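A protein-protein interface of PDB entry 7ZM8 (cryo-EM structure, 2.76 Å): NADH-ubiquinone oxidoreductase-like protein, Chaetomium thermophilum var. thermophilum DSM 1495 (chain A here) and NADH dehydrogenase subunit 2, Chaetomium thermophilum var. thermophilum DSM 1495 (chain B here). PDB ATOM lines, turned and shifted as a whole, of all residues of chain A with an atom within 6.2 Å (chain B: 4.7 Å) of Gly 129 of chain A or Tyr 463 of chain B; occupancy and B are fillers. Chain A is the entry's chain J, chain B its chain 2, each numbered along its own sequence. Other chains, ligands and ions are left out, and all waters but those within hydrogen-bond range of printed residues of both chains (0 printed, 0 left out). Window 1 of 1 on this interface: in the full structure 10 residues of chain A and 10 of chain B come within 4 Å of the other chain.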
ATOM      1  N   ALA A 123      18.355   7.749  15.179  1.00  0.00           N
ATOM      2  CA  ALA A 123      16.917   7.727  14.954  1.00  0.00           C
ATOM      3  C   ALA A 123      16.164   7.418  16.239  1.00  0.00           C
ATOM      4  O   ALA A 123      15.147   8.050  16.537  1.00  0.00           O
ATOM      5  CB  ALA A 123      16.573   6.706  13.874  1.00  0.00           C
ATOM      6  N   GLY A 127      13.819   9.923  18.602  1.00  0.00           N
ATOM      7  CA  GLY A 127      12.395   9.549  18.700  1.00  0.00           C
ATOM      8  C   GLY A 127      11.954   9.029  17.347  1.00  0.00           C
ATOM      9  O   GLY A 127      12.579   9.437  16.349  1.00  0.00           O
ATOM     10  N   SER A 128      10.933   8.169  17.288  1.00  0.00           N
ATOM     11  CA  SER A 128      10.609   7.579  15.961  1.00  0.00           C
ATOM     12  C   SER A 128       9.956   8.613  15.041  1.00  0.00           C
ATOM     13  O   SER A 128       8.741   8.852  15.188  1.00  0.00           O
ATOM     14  CB  SER A 128       9.729   6.368  16.124  1.00  0.00           C
ATOM     15  OG  SER A 128      10.322   5.425  17.005  1.00  0.00           O
ATOM     16  N   GLY A 129      10.739   9.199  14.127  1.00  0.00           N
ATOM     17  CA  GLY A 129      10.199  10.145  13.132  1.00  0.00           C
ATOM     18  C   GLY A 129       9.354   9.449  12.083  1.00  0.00           C
ATOM     19  O   GLY A 129       8.335  10.032  11.675  1.00  0.00           O
ATOM     20  N   LEU A 130       9.761   8.252  11.646  1.00  0.00           N
ATOM     21  CA  LEU A 130       9.059   7.561  10.527  1.00  0.00           C
ATOM     22  C   LEU A 130       7.624   7.166  10.897  1.00  0.00           C
ATOM     23  O   LEU A 130       6.829   6.950   9.968  1.00  0.00           O
ATOM     24  CB  LEU A 130       9.907   6.380  10.052  1.00  0.00           C
ATOM     25  CG  LEU A 130      11.280   6.760   9.497  1.00  0.00           C
ATOM     26  CD1 LEU A 130      12.046   5.527   9.048  1.00  0.00           C
ATOM     27  CD2 LEU A 130      11.143   7.749   8.350  1.00  0.00           C
ATOM     28  N   ARG A 131       7.307   7.038  12.184  1.00  0.00           N
ATOM     29  CA  ARG A 131       5.926   6.810  12.573  1.00  0.00           C
ATOM     30  C   ARG A 131       5.380   8.086  13.209  1.00  0.00           C
ATOM     31  O   ARG A 131       6.027   9.139  13.195  1.00  0.00           O
ATOM     32  CB  ARG A 131       5.821   5.615  13.521  1.00  0.00           C
ATOM     33  CG  ARG A 131       6.586   4.390  13.068  1.00  0.00           C
ATOM     34  CD  ARG A 131       5.984   3.797  11.810  1.00  0.00           C
ATOM     35  NE  ARG A 131       4.684   3.182  12.056  1.00  0.00           N
ATOM     36  CZ  ARG A 131       3.950   2.596  11.117  1.00  0.00           C
ATOM     37  NH1 ARG A 131       4.389   2.542   9.868  1.00  0.00           N
ATOM     38  NH2 ARG A 131       2.779   2.059  11.427  1.00  0.00           N
ATOM     39  N   GLY A 132       4.178   8.003  13.767  1.00  0.00           N
ATOM     40  CA  GLY A 132       3.626   9.120  14.504  1.00  0.00           C
ATOM     41  C   GLY A 132       4.461   9.454  15.721  1.00  0.00           C
ATOM     42  O   GLY A 132       4.716   8.586  16.562  1.00  0.00           O
ATOM     43  N   VAL A 133       4.900  10.709  15.825  1.00  0.00           N
ATOM     44  CA  VAL A 133       5.734  11.114  16.949  1.00  0.00           C
ATOM     45  C   VAL A 133       4.916  11.072  18.234  1.00  0.00           C
ATOM     46  O   VAL A 133       3.689  11.244  18.229  1.00  0.00           O
ATOM     47  CB  VAL A 133       6.333  12.511  16.706  1.00  0.00           C
ATOM     48  CG1 VAL A 133       5.273  13.590  16.864  1.00  0.00           C
ATOM     49  CG2 VAL A 133       7.514  12.762  17.635  1.00  0.00           C
ATOM     50  N   LEU B 316       6.250  11.043   4.509  1.00  0.00           N
ATOM     51  CA  LEU B 316       7.486  11.151   5.332  1.00  0.00           C
ATOM     52  C   LEU B 316       8.612  10.286   4.759  1.00  0.00           C
ATOM     53  O   LEU B 316       9.776  10.657   4.914  1.00  0.00           O
ATOM     54  CB  LEU B 316       7.211  10.790   6.788  1.00  0.00           C
ATOM     55  CG  LEU B 316       7.066  11.956   7.755  1.00  0.00           C
ATOM     56  CD1 LEU B 316       6.996  11.429   9.174  1.00  0.00           C
ATOM     57  CD2 LEU B 316       8.222  12.929   7.610  1.00  0.00           C
ATOM     58  N   SER B 356       3.904  16.698   5.993  1.00  0.00           N
ATOM     59  CA  SER B 356       3.770  15.520   6.891  1.00  0.00           C
ATOM     60  C   SER B 356       3.725  15.940   8.361  1.00  0.00           C
ATOM     61  O   SER B 356       3.058  15.255   9.146  1.00  0.00           O
ATOM     62  CB  SER B 356       4.881  14.551   6.636  1.00  0.00           C
ATOM     63  OG  SER B 356       4.885  14.138   5.283  1.00  0.00           O
ATOM     64  N   VAL B 357       4.424  17.011   8.722  1.00  0.00           N
ATOM     65  CA  VAL B 357       4.308  17.521  10.112  1.00  0.00           C
ATOM     66  C   VAL B 357       3.072  18.411  10.078  1.00  0.00           C
ATOM     67  O   VAL B 357       3.144  19.465   9.459  1.00  0.00           O
ATOM     68  CB  VAL B 357       5.551  18.352  10.480  1.00  0.00           C
ATOM     69  CG1 VAL B 357       5.515  18.859  11.910  1.00  0.00           C
ATOM     70  CG2 VAL B 357       6.848  17.621  10.182  1.00  0.00           C
ATOM     71  N   ALA B 458       9.859  21.357  11.824  1.00  0.00           N
ATOM     72  CA  ALA B 458      10.157  19.936  12.091  1.00  0.00           C
ATOM     73  C   ALA B 458      10.866  19.785  13.434  1.00  0.00           C
ATOM     74  O   ALA B 458      10.491  18.879  14.190  1.00  0.00           O
ATOM     75  CB  ALA B 458      11.008  19.419  10.972  1.00  0.00           C
ATOM     76  N   LEU B 459      11.829  20.660  13.726  1.00  0.00           N
ATOM     77  CA  LEU B 459      12.613  20.558  14.980  1.00  0.00           C
ATOM     78  C   LEU B 459      11.688  20.736  16.179  1.00  0.00           C
ATOM     79  O   LEU B 459      11.840  19.985  17.151  1.00  0.00           O
ATOM     80  CB  LEU B 459      13.665  21.671  14.963  1.00  0.00           C
ATOM     81  CG  LEU B 459      14.965  21.372  14.223  1.00  0.00           C
ATOM     82  CD1 LEU B 459      15.813  22.631  14.153  1.00  0.00           C
ATOM     83  CD2 LEU B 459      15.729  20.248  14.901  1.00  0.00           C
ATOM     84  N   ASN B 461       8.633  20.055  16.449  1.00  0.00           N
ATOM     85  CA  ASN B 461       7.619  18.973  16.571  1.00  0.00           C
ATOM     86  C   ASN B 461       8.273  17.608  16.810  1.00  0.00           C
ATOM     87  O   ASN B 461       7.528  16.631  16.986  1.00  0.00           O
ATOM     88  CB  ASN B 461       6.633  18.962  15.407  1.00  0.00           C
ATOM     89  CG  ASN B 461       5.198  19.111  15.863  1.00  0.00           C
ATOM     90  OD1 ASN B 461       4.927  19.780  16.856  1.00  0.00           O
ATOM     91  ND2 ASN B 461       4.275  18.496  15.144  1.00  0.00           N
ATOM     92  N   GLY B 462       9.601  17.536  16.815  1.00  0.00           N
ATOM     93  CA  GLY B 462      10.278  16.268  17.132  1.00  0.00           C
ATOM     94  C   GLY B 462      10.780  15.538  15.902  1.00  0.00           C
ATOM     95  O   GLY B 462      11.121  14.352  16.025  1.00  0.00           O
ATOM     96  N   TYR B 463      10.824  16.212  14.757  1.00  0.00           N
ATOM     97  CA  TYR B 463      11.388  15.587  13.532  1.00  0.00           C
ATOM     98  C   TYR B 463      12.857  16.001  13.414  1.00  0.00           C
ATOM     99  O   TYR B 463      13.264  16.471  12.346  1.00  0.00           O
ATOM    100  CB  TYR B 463      10.520  15.872  12.305  1.00  0.00           C
ATOM    101  CG  TYR B 463       9.091  15.399  12.389  1.00  0.00           C
ATOM    102  CD1 TYR B 463       8.160  16.057  13.175  1.00  0.00           C
ATOM    103  CD2 TYR B 463       8.659  14.307  11.659  1.00  0.00           C
ATOM    104  CE1 TYR B 463       6.845  15.631  13.254  1.00  0.00           C
ATOM    105  CE2 TYR B 463       7.346  13.870  11.720  1.00  0.00           C
ATOM    106  CZ  TYR B 463       6.435  14.536  12.518  1.00  0.00           C
ATOM    107  OH  TYR B 463       5.141  14.109  12.581  1.00  0.00           O
ATOM    108  N   ILE B 464      13.617  15.806  14.492  1.00  0.00           N
ATOM    109  CA  ILE B 464      15.057  16.185  14.541  1.00  0.00           C
ATOM    110  C   ILE B 464      15.861  15.266  13.619  1.00  0.00           C
ATOM    111  O   ILE B 464      16.768  15.775  12.932  1.00  0.00           O
ATOM    112  CB  ILE B 464      15.544  16.157  16.005  1.00  0.00           C
ATOM    113  CG1 ILE B 464      17.053  15.929  16.132  1.00  0.00           C
ATOM    114  CG2 ILE B 464      14.744  15.159  16.828  1.00  0.00           C
ATOM    115  CD1 ILE B 464      17.876  17.194  16.052  1.00  0.00           C
ATOM    116  N   PHE B 465      15.538  13.972  13.590  1.00  0.00           N
ATOM    117  CA  PHE B 465      16.341  13.029  12.766  1.00  0.00           C
ATOM    118  C   PHE B 465      16.197  13.414  11.292  1.00  0.00           C
ATOM    119  O   PHE B 465      17.212  13.428  10.583  1.00  0.00           O
ATOM    120  CB  PHE B 465      15.982  11.574  13.080  1.00  0.00           C
ATOM    121  CG  PHE B 465      16.510  10.579  12.079  1.00  0.00           C
ATOM    122  CD1 PHE B 465      17.831  10.168  12.120  1.00  0.00           C
ATOM    123  CD2 PHE B 465      15.692  10.070  11.084  1.00  0.00           C
ATOM    124  CE1 PHE B 465      18.319   9.264  11.193  1.00  0.00           C
ATOM    125  CE2 PHE B 465      16.183   9.168  10.155  1.00  0.00           C
ATOM    126  CZ  PHE B 465      17.495   8.765  10.213  1.00  0.00           C
ATOM    127  N   LEU B 466      14.979  13.732  10.861  1.00  0.00           N
ATOM    128  CA  LEU B 466      14.726  14.166   9.462  1.00  0.00           C
ATOM    129  C   LEU B 466      15.409  15.499   9.150  1.00  0.00           C
ATOM    130  O   LEU B 466      15.904  15.641   8.024  1.00  0.00           O
ATOM    131  CB  LEU B 466      13.215  14.227   9.231  1.00  0.00           C
ATOM    132  CG  LEU B 466      12.587  12.890   8.846  1.00  0.00           C
ATOM    133  CD1 LEU B 466      11.228  12.713   9.503  1.00  0.00           C
ATOM    134  CD2 LEU B 466      12.489  12.747   7.337  1.00  0.00           C
ATOM    135  N   SER B 467      15.413  16.436  10.097  1.00  0.00           N
ATOM    136  CA  SER B 467      16.051  17.763   9.897  1.00  0.00           C
ATOM    137  C   SER B 467      17.556  17.599   9.666  1.00  0.00           C
ATOM    138  O   SER B 467      18.100  18.319   8.817  1.00  0.00           O
ATOM    139  CB  SER B 467      15.776  18.678  11.062  1.00  0.00           C
ATOM    140  OG  SER B 467      14.382  18.841  11.266  1.00  0.00           O
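The backbone carbonyl oxygen (O) of Ala 458 of chain B sits at hydrogen-bond distance from the backbone NH (N) of Tyr 463 of chain B, at 2.7 Å.
N of Leu 316 of chain B sits at hydrogen-bond distance from OG of Ser 356 of chain B, at 3.5 Å.
The backbone carbonyl oxygen (O) of Tyr 463 of chain B is in hydrogen-bond range of the side-chain hydroxyl (OG) of Ser 467 of chain B (2.8 Å).
Phe 465 of chain B touches Ala 123 of chain A (CD1 to CA, 3.9 Å).
Gly 129 of chain A touches Leu 316 of chain B.
Tyr 463 of chain B touches Gly 129 of chain A (CE2 to O, 3.96 Å).
Asn 461 of chain B touches Val 133 of chain A.
Printed residues of chain B within 4 Å of Ala 123 of chain A: Phe 465 (3.9 Å).
Of chain B, only Leu 316 and Tyr 463 come within 4 Å of Gly 129 of chain A.
Printed residues of chain B within 4 Å of Val 133 of chain A: Asn 461.
Printed residues of chain A within 4 Å of Leu 316 of chain B: Gly 129 (3.2 Å).
Gly 462 of chain B touches none of the printed residues of chain A.
Tyr 463 of chain B touches one residue of chain A.
Ser 467 of chain B touches none of the printed residues of chain A.
The nearest residue of chain A that does not touch Tyr 463 of chain B is Val 133 of chain A (4.3 Å).
Printed residues of chain A that touch a printed residue of chain B: Ala 123, Gly 129 and Val 133.
Hydrophobic or aromatic side chains of chain A within 4 Å of the printed part of chain B: Val 133.
Of the 12 printed residues of chain B, 4 touch a printed residue of chain A.
Hydrophobic or aromatic side chains of chain B that line the printed part of chain A: Leu 316, Tyr 463 and Phe 465.
Among the printed residues, 4 pairs touch across the chains.
Among the printed residues, no Asp or Glu carboxylate lies within 4 Å of a Lys or Arg side-chain nitrogen of the other chain.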
